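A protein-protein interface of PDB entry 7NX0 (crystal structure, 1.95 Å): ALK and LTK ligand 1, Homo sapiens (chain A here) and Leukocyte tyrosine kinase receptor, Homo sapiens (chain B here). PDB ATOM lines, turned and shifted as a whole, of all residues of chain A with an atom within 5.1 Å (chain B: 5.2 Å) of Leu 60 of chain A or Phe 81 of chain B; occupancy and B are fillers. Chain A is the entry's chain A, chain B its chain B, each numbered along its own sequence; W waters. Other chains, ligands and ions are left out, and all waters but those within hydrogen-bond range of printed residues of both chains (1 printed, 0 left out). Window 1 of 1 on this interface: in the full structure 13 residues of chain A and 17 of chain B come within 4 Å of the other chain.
NE of Arg 59 of chain A is in hydrogen-bond range of O of Val 304 of chain B (2.8 Å).
OE2 of Glu 47 of chain A is in hydrogen-bond range of OH of Tyr 62 of chain B (2.6 Å).
N of Leu 299 of chain B sits at hydrogen-bond distance from OG of Ser 83 of chain B.
O of Leu 41 of chain A sits at hydrogen-bond distance from OG1 of Thr 45 of chain A (2.7 Å).
O of Leu 302 of chain B is in hydrogen-bond range of N of Phe 81 of chain B (2.8 Å).
The backbone carbonyl oxygen of Gly 79 of chain B sits at hydrogen-bond distance from the backbone NH of Val 304 of chain B, 2.9 Å away.
Among the printed residues, pairs that only touch across the chains: Arg 63 of chain A with Ala 303 of chain B, Leu 60 of chain A with Val 304 of chain B, Leu 64 of chain A with Gln 300 of chain B, Leu 64 of chain A with Leu 302 of chain B, Arg 56 of chain A with Val 304 of chain B, Arg 63 of chain A with Leu 302 of chain B, Leu 60 of chain A with Leu 302 of chain B, Thr 45 of chain A with Leu 299 of chain B, Leu 60 of chain A with Phe 81 of chain B and Leu 41 of chain A with Leu 299 of chain B.
Of chain B, only Phe 81 (3.9 Å), Leu 302 (3.8 Å) and Val 304 (3.4 Å) come within 4 Å of Leu 60 of chain A.
Printed residues of chain B within 4 Å of Leu 64 of chain A: Gln 300 (3.5 Å) and Leu 302 (3.5 Å).
Printed residues of chain A within 4 Å of Phe 81 of chain B: Leu 60.
Ala 169 of chain B touches none of the printed residues of chain A.
Pro 301 of chain B touches none of the printed residues of chain A.
Of the printed residues of chain A, Leu 302 of chain B touches Leu 60 (3.8 Å), Arg 63 (3.7 Å) and Leu 64 (3.5 Å).
Of the 13 printed residues of chain A, 8 touch a printed residue of chain B.
Hydrophobic or aromatic side chains of chain A within 4 Å of the printed part of chain B: Leu 41, Leu 60 and Leu 64.
Of the 16 printed residues of chain B, 7 touch a printed residue of chain A.
Hydrophobic or aromatic side chains of chain B within 4 Å of the printed part of chain A: Tyr 62, Phe 81, Leu 299, Leu 302 and Val 304.
Among the printed residues, 12 pairs touch across the chains.
Among the printed residues, no Asp or Glu carboxylate lies within 4 Å of a Lys or Arg side-chain nitrogen of the other chain.
Water W1 bridges OE1 of Glu 47 of chain A (2.9 Å) and OH of Tyr 62 of chain B (3.4 Å).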
ATOM      1  N   LEU A  41       7.074  -3.046  25.985  1.00  0.00           N
ATOM      2  CA  LEU A  41       5.750  -3.391  25.487  1.00  0.00           C
ATOM      3  C   LEU A  41       5.805  -4.628  24.602  1.00  0.00           C
ATOM      4  O   LEU A  41       4.994  -5.549  24.749  1.00  0.00           O
ATOM      5  CB  LEU A  41       5.183  -2.206  24.722  1.00  0.00           C
ATOM      6  CG  LEU A  41       3.772  -2.327  24.159  1.00  0.00           C
ATOM      7  CD1 LEU A  41       2.808  -2.748  25.222  1.00  0.00           C
ATOM      8  CD2 LEU A  41       3.404  -0.972  23.575  1.00  0.00           C
ATOM      9  N   THR A  45       5.033  -7.778  27.936  1.00  0.00           N
ATOM     10  CA  THR A  45       3.624  -7.679  28.292  1.00  0.00           C
ATOM     11  C   THR A  45       2.896  -8.955  27.889  1.00  0.00           C
ATOM     12  O   THR A  45       3.310  -9.660  26.963  1.00  0.00           O
ATOM     13  CB  THR A  45       2.925  -6.484  27.619  1.00  0.00           C
ATOM     14  OG1 THR A  45       2.961  -6.630  26.193  1.00  0.00           O
ATOM     15  CG2 THR A  45       3.577  -5.167  28.031  1.00  0.00           C
ATOM     16  N   GLU A  47       0.143  -8.898  26.411  1.00  0.00           N
ATOM     17  CA  GLU A  47      -0.558  -8.633  25.158  1.00  0.00           C
ATOM     18  C   GLU A  47       0.281  -9.014  23.950  1.00  0.00           C
ATOM     19  O   GLU A  47      -0.230  -9.607  22.993  1.00  0.00           O
ATOM     20  CB  GLU A  47      -0.936  -7.155  25.053  1.00  0.00           C
ATOM     21  CG  GLU A  47      -2.203  -6.771  25.762  1.00  0.00           C
ATOM     22  CD  GLU A  47      -1.992  -6.551  27.240  1.00  0.00           C
ATOM     23  OE1 GLU A  47      -0.854  -6.749  27.721  1.00  0.00           O
ATOM     24  OE2 GLU A  47      -2.967  -6.175  27.918  1.00  0.00           O
ATOM     25  N   ARG A  56      -4.746  -6.573  20.662  1.00  0.00           N
ATOM     26  CA  ARG A  56      -4.428  -5.681  21.771  1.00  0.00           C
ATOM     27  C   ARG A  56      -2.998  -5.174  21.667  1.00  0.00           C
ATOM     28  O   ARG A  56      -2.739  -3.984  21.868  1.00  0.00           O
ATOM     29  CB  ARG A  56      -4.638  -6.397  23.102  1.00  0.00           C
ATOM     30  CG  ARG A  56      -6.085  -6.666  23.455  1.00  0.00           C
ATOM     31  CD  ARG A  56      -6.199  -7.290  24.837  1.00  0.00           C
ATOM     32  NE  ARG A  56      -7.406  -8.096  24.973  1.00  0.00           N
ATOM     33  CZ  ARG A  56      -7.777  -8.720  26.087  1.00  0.00           C
ATOM     34  NH1 ARG A  56      -7.036  -8.635  27.187  1.00  0.00           N
ATOM     35  NH2 ARG A  56      -8.893  -9.435  26.100  1.00  0.00           N
ATOM     36  N   CYS A  57      -2.049  -6.063  21.360  1.00  0.00           N
ATOM     37  CA  CYS A  57      -0.672  -5.620  21.183  1.00  0.00           C
ATOM     38  C   CYS A  57      -0.608  -4.481  20.175  1.00  0.00           C
ATOM     39  O   CYS A  57       0.006  -3.437  20.428  1.00  0.00           O
ATOM     40  CB  CYS A  57       0.211  -6.790  20.730  1.00  0.00           C
ATOM     41  SG  CYS A  57       1.973  -6.401  20.506  1.00  0.00           S
ATOM     42  N   ALA A  58      -1.281  -4.652  19.036  1.00  0.00           N
ATOM     43  CA  ALA A  58      -1.187  -3.669  17.961  1.00  0.00           C
ATOM     44  C   ALA A  58      -1.796  -2.328  18.364  1.00  0.00           C
ATOM     45  O   ALA A  58      -1.277  -1.275  17.980  1.00  0.00           O
ATOM     46  CB  ALA A  58      -1.860  -4.208  16.699  1.00  0.00           C
ATOM     47  N   ARG A  59      -2.895  -2.339  19.125  1.00  0.00           N
ATOM     48  CA  ARG A  59      -3.450  -1.071  19.594  1.00  0.00           C
ATOM     49  C   ARG A  59      -2.455  -0.366  20.508  1.00  0.00           C
ATOM     50  O   ARG A  59      -2.164   0.820  20.336  1.00  0.00           O
ATOM     51  CB  ARG A  59      -4.777  -1.301  20.318  1.00  0.00           C
ATOM     52  CG  ARG A  59      -5.877  -1.799  19.403  1.00  0.00           C
ATOM     53  CD  ARG A  59      -7.251  -1.476  19.945  1.00  0.00           C
ATOM     54  NE  ARG A  59      -7.657  -2.337  21.052  1.00  0.00           N
ATOM     55  CZ  ARG A  59      -8.191  -3.547  20.902  1.00  0.00           C
ATOM     56  NH1 ARG A  59      -8.369  -4.048  19.688  1.00  0.00           N
ATOM     57  NH2 ARG A  59      -8.544  -4.256  21.968  1.00  0.00           N
ATOM     58  N   LEU A  60      -1.899  -1.108  21.464  1.00  0.00           N
ATOM     59  CA  LEU A  60      -0.917  -0.549  22.388  1.00  0.00           C
ATOM     60  C   LEU A  60       0.267   0.051  21.642  1.00  0.00           C
ATOM     61  O   LEU A  60       0.673   1.191  21.909  1.00  0.00           O
ATOM     62  CB  LEU A  60      -0.434  -1.639  23.344  1.00  0.00           C
ATOM     63  CG  LEU A  60      -1.415  -2.251  24.335  1.00  0.00           C
ATOM     64  CD1 LEU A  60      -0.787  -3.398  25.094  1.00  0.00           C
ATOM     65  CD2 LEU A  60      -1.840  -1.125  25.254  1.00  0.00           C
ATOM     66  N   LEU A  61       0.865  -0.730  20.733  1.00  0.00           N
ATOM     67  CA  LEU A  61       1.962  -0.218  19.919  1.00  0.00           C
ATOM     68  C   LEU A  61       1.533   1.019  19.144  1.00  0.00           C
ATOM     69  O   LEU A  61       2.306   1.975  19.001  1.00  0.00           O
ATOM     70  CB  LEU A  61       2.445  -1.297  18.955  1.00  0.00           C
ATOM     71  CG  LEU A  61       3.162  -2.503  19.559  1.00  0.00           C
ATOM     72  CD1 LEU A  61       3.325  -3.606  18.514  1.00  0.00           C
ATOM     73  CD2 LEU A  61       4.517  -2.092  20.110  1.00  0.00           C
ATOM     74  N   THR A  62       0.310   1.008  18.612  1.00  0.00           N
ATOM     75  CA  THR A  62      -0.188   2.179  17.905  1.00  0.00           C
ATOM     76  C   THR A  62      -0.286   3.374  18.844  1.00  0.00           C
ATOM     77  O   THR A  62       0.057   4.500  18.467  1.00  0.00           O
ATOM     78  CB  THR A  62      -1.543   1.860  17.270  1.00  0.00           C
ATOM     79  OG1 THR A  62      -1.382   0.813  16.298  1.00  0.00           O
ATOM     80  CG2 THR A  62      -2.124   3.089  16.594  1.00  0.00           C
ATOM     81  N   ARG A  63      -0.726   3.145  20.082  1.00  0.00           N
ATOM     82  CA  ARG A  63      -0.861   4.253  21.021  1.00  0.00           C
ATOM     83  C   ARG A  63       0.498   4.755  21.486  1.00  0.00           C
ATOM     84  O   ARG A  63       0.675   5.963  21.673  1.00  0.00           O
ATOM     85  CB  ARG A  63      -1.723   3.827  22.212  1.00  0.00           C
ATOM     86  CG  ARG A  63      -3.183   3.508  21.854  1.00  0.00           C
ATOM     87  CD  ARG A  63      -3.820   4.619  21.023  1.00  0.00           C
ATOM     88  NE  ARG A  63      -3.750   5.919  21.682  1.00  0.00           N
ATOM     89  CZ  ARG A  63      -3.996   7.075  21.072  1.00  0.00           C
ATOM     90  NH1 ARG A  63      -4.323   7.093  19.786  1.00  0.00           N
ATOM     91  NH2 ARG A  63      -3.906   8.215  21.742  1.00  0.00           N
ATOM     92  N   LEU A  64       1.472   3.858  21.653  1.00  0.00           N
ATOM     93  CA  LEU A  64       2.818   4.296  22.003  1.00  0.00           C
ATOM     94  C   LEU A  64       3.415   5.152  20.892  1.00  0.00           C
ATOM     95  O   LEU A  64       3.971   6.224  21.156  1.00  0.00           O
ATOM     96  CB  LEU A  64       3.696   3.080  22.303  1.00  0.00           C
ATOM     97  CG  LEU A  64       5.131   3.345  22.765  1.00  0.00           C
ATOM     98  CD1 LEU A  64       5.177   4.084  24.096  1.00  0.00           C
ATOM     99  CD2 LEU A  64       5.919   2.031  22.866  1.00  0.00           C
ATOM    100  N   ALA A  65       3.269   4.718  19.636  1.00  0.00           N
ATOM    101  CA  ALA A  65       3.927   5.407  18.528  1.00  0.00           C
ATOM    102  C   ALA A  65       3.457   6.849  18.379  1.00  0.00           C
ATOM    103  O   ALA A  65       4.247   7.717  17.983  1.00  0.00           O
ATOM    104  CB  ALA A  65       3.693   4.644  17.224  1.00  0.00           C
ATOM    105  N   SER B  60      -0.793  -3.947  36.663  1.00  0.00           N
ATOM    106  CA  SER B  60      -1.268  -3.519  35.357  1.00  0.00           C
ATOM    107  C   SER B  60      -2.772  -3.329  35.462  1.00  0.00           C
ATOM    108  O   SER B  60      -3.512  -4.302  35.628  1.00  0.00           O
ATOM    109  CB  SER B  60      -0.913  -4.551  34.290  1.00  0.00           C
ATOM    110  OG  SER B  60       0.482  -4.575  34.078  1.00  0.00           O
ATOM    111  N   ALA B  61      -3.221  -2.081  35.381  1.00  0.00           N
ATOM    112  CA  ALA B  61      -4.634  -1.752  35.483  1.00  0.00           C
ATOM    113  C   ALA B  61      -5.159  -1.286  34.129  1.00  0.00           C
ATOM    114  O   ALA B  61      -4.491  -0.523  33.422  1.00  0.00           O
ATOM    115  CB  ALA B  61      -4.870  -0.678  36.546  1.00  0.00           C
ATOM    116  N   TYR B  62      -6.357  -1.757  33.783  1.00  0.00           N
ATOM    117  CA  TYR B  62      -7.010  -1.450  32.512  1.00  0.00           C
ATOM    118  C   TYR B  62      -8.388  -0.877  32.810  1.00  0.00           C
ATOM    119  O   TYR B  62      -9.221  -1.564  33.412  1.00  0.00           O
ATOM    120  CB  TYR B  62      -7.157  -2.700  31.632  1.00  0.00           C
ATOM    121  CG  TYR B  62      -5.874  -3.420  31.283  1.00  0.00           C
ATOM    122  CD1 TYR B  62      -5.224  -4.214  32.219  1.00  0.00           C
ATOM    123  CD2 TYR B  62      -5.336  -3.336  30.007  1.00  0.00           C
ATOM    124  CE1 TYR B  62      -4.057  -4.886  31.900  1.00  0.00           C
ATOM    125  CE2 TYR B  62      -4.167  -4.005  29.678  1.00  0.00           C
ATOM    126  CZ  TYR B  62      -3.532  -4.776  30.635  1.00  0.00           C
ATOM    127  OH  TYR B  62      -2.373  -5.446  30.325  1.00  0.00           O
ATOM    128  N   GLY B  63      -8.630   0.370  32.403  1.00  0.00           N
ATOM    129  CA  GLY B  63      -9.969   0.927  32.481  1.00  0.00           C
ATOM    130  C   GLY B  63     -10.872   0.337  31.417  1.00  0.00           C
ATOM    131  O   GLY B  63     -10.432  -0.398  30.536  1.00  0.00           O
ATOM    132  N   GLY B  79     -10.698   1.777  26.932  1.00  0.00           N
ATOM    133  CA  GLY B  79     -10.189   2.029  28.265  1.00  0.00           C
ATOM    134  C   GLY B  79      -8.674   1.989  28.294  1.00  0.00           C
ATOM    135  O   GLY B  79      -8.025   1.339  27.468  1.00  0.00           O
ATOM    136  N   VAL B  80      -8.100   2.692  29.253  1.00  0.00           N
ATOM    137  CA  VAL B  80      -6.670   2.953  29.264  1.00  0.00           C
ATOM    138  C   VAL B  80      -5.958   1.931  30.136  1.00  0.00           C
ATOM    139  O   VAL B  80      -6.460   1.533  31.193  1.00  0.00           O
ATOM    140  CB  VAL B  80      -6.370   4.385  29.740  1.00  0.00           C
ATOM    141  CG1 VAL B  80      -4.876   4.593  29.844  1.00  0.00           C
ATOM    142  CG2 VAL B  80      -6.997   5.386  28.779  1.00  0.00           C
ATOM    143  N   PHE B  81      -4.785   1.509  29.673  1.00  0.00           N
ATOM    144  CA  PHE B  81      -3.864   0.639  30.389  1.00  0.00           C
ATOM    145  C   PHE B  81      -2.778   1.493  31.022  1.00  0.00           C
ATOM    146  O   PHE B  81      -2.159   2.311  30.340  1.00  0.00           O
ATOM    147  CB  PHE B  81      -3.286  -0.375  29.391  1.00  0.00           C
ATOM    148  CG  PHE B  81      -2.012  -1.047  29.834  1.00  0.00           C
ATOM    149  CD1 PHE B  81      -1.958  -1.760  31.018  1.00  0.00           C
ATOM    150  CD2 PHE B  81      -0.883  -0.999  29.037  1.00  0.00           C
ATOM    151  CE1 PHE B  81      -0.787  -2.392  31.409  1.00  0.00           C
ATOM    152  CE2 PHE B  81       0.293  -1.627  29.428  1.00  0.00           C
ATOM    153  CZ  PHE B  81       0.336  -2.326  30.610  1.00  0.00           C
ATOM    154  N   VAL B  82      -2.594   1.344  32.337  1.00  0.00           N
ATOM    155  CA  VAL B  82      -1.461   1.923  33.047  1.00  0.00           C
ATOM    156  C   VAL B  82      -0.846   0.832  33.916  1.00  0.00           C
ATOM    157  O   VAL B  82      -1.525  -0.119  34.318  1.00  0.00           O
ATOM    158  CB  VAL B  82      -1.821   3.149  33.933  1.00  0.00           C
ATOM    159  CG1 VAL B  82      -2.217   4.358  33.080  1.00  0.00           C
ATOM    160  CG2 VAL B  82      -2.886   2.789  34.965  1.00  0.00           C
ATOM    161  N   SER B  83       0.435   0.983  34.230  1.00  0.00           N
ATOM    162  CA  SER B  83       1.149  -0.036  34.986  1.00  0.00           C
ATOM    163  C   SER B  83       2.320   0.587  35.722  1.00  0.00           C
ATOM    164  O   SER B  83       2.972   1.502  35.215  1.00  0.00           O
ATOM    165  CB  SER B  83       1.645  -1.149  34.057  1.00  0.00           C
ATOM    166  OG  SER B  83       2.387  -0.604  32.982  1.00  0.00           O
ATOM    167  N   ALA B 169      -6.812   3.614  36.128  1.00  0.00           N
ATOM    168  CA  ALA B 169      -6.782   3.422  34.680  1.00  0.00           C
ATOM    169  C   ALA B 169      -8.079   3.981  34.104  1.00  0.00           C
ATOM    170  O   ALA B 169      -9.157   3.437  34.361  1.00  0.00           O
ATOM    171  CB  ALA B 169      -6.621   1.943  34.344  1.00  0.00           C
ATOM    172  N   LEU B 299       4.922   1.246  32.164  1.00  0.00           N
ATOM    173  CA  LEU B 299       4.548   1.767  30.860  1.00  0.00           C
ATOM    174  C   LEU B 299       3.545   2.897  31.049  1.00  0.00           C
ATOM    175  O   LEU B 299       2.705   2.864  31.951  1.00  0.00           O
ATOM    176  CB  LEU B 299       3.947   0.676  29.969  1.00  0.00           C
ATOM    177  CG  LEU B 299       4.929  -0.365  29.440  1.00  0.00           C
ATOM    178  CD1 LEU B 299       4.195  -1.486  28.719  1.00  0.00           C
ATOM    179  CD2 LEU B 299       5.954   0.292  28.521  1.00  0.00           C
ATOM    180  N   GLN B 300       3.637   3.885  30.188  1.00  0.00           N
ATOM    181  CA  GLN B 300       2.742   5.033  30.225  1.00  0.00           C
ATOM    182  C   GLN B 300       1.303   4.641  29.917  1.00  0.00           C
ATOM    183  O   GLN B 300       1.050   3.507  29.488  1.00  0.00           O
ATOM    184  CB  GLN B 300       3.221   6.073  29.219  1.00  0.00           C
ATOM    185  CG  GLN B 300       3.031   5.617  27.789  1.00  0.00           C
ATOM    186  CD  GLN B 300       4.014   6.247  26.837  1.00  0.00           C
ATOM    187  OE1 GLN B 300       5.221   6.042  26.951  1.00  0.00           O
ATOM    188  NE2 GLN B 300       3.505   7.022  25.891  1.00  0.00           N
ATOM    189  N   PRO B 301       0.340   5.541  30.135  1.00  0.00           N
ATOM    190  CA  PRO B 301      -1.051   5.226  29.790  1.00  0.00           C
ATOM    191  C   PRO B 301      -1.207   4.977  28.296  1.00  0.00           C
ATOM    192  O   PRO B 301      -0.690   5.734  27.471  1.00  0.00           O
ATOM    193  CB  PRO B 301      -1.824   6.473  30.234  1.00  0.00           C
ATOM    194  CG  PRO B 301      -0.921   7.173  31.209  1.00  0.00           C
ATOM    195  CD  PRO B 301       0.481   6.866  30.765  1.00  0.00           C
ATOM    196  N   LEU B 302      -1.928   3.905  27.955  1.00  0.00           N
ATOM    197  CA  LEU B 302      -2.175   3.526  26.565  1.00  0.00           C
ATOM    198  C   LEU B 302      -3.579   2.963  26.420  1.00  0.00           C
ATOM    199  O   LEU B 302      -3.892   1.925  27.012  1.00  0.00           O
ATOM    200  CB  LEU B 302      -1.159   2.487  26.089  1.00  0.00           C
ATOM    201  CG  LEU B 302       0.298   2.912  26.160  1.00  0.00           C
ATOM    202  CD1 LEU B 302       1.208   1.701  26.008  1.00  0.00           C
ATOM    203  CD2 LEU B 302       0.620   3.940  25.095  1.00  0.00           C
ATOM    204  N   ALA B 303      -4.408   3.613  25.602  1.00  0.00           N
ATOM    205  CA  ALA B 303      -5.776   3.148  25.385  1.00  0.00           C
ATOM    206  C   ALA B 303      -5.772   1.829  24.624  1.00  0.00           C
ATOM    207  O   ALA B 303      -5.234   1.755  23.518  1.00  0.00           O
ATOM    208  CB  ALA B 303      -6.573   4.196  24.611  1.00  0.00           C
ATOM    209  N   VAL B 304      -6.302   0.765  25.234  1.00  0.00           N
ATOM    210  CA  VAL B 304      -6.378  -0.508  24.517  1.00  0.00           C
ATOM    211  C   VAL B 304      -7.671  -1.293  24.702  1.00  0.00           C
ATOM    212  O   VAL B 304      -8.058  -2.081  23.837  1.00  0.00           O
ATOM    213  CB  VAL B 304      -5.188  -1.390  24.928  1.00  0.00           C
ATOM    214  CG1 VAL B 304      -5.197  -1.564  26.455  1.00  0.00           C
ATOM    215  CG2 VAL B 304      -5.237  -2.739  24.232  1.00  0.00           C
HETATM  216  O   HOH W   1      -0.611  -3.841  27.900  1.00  0.00           O
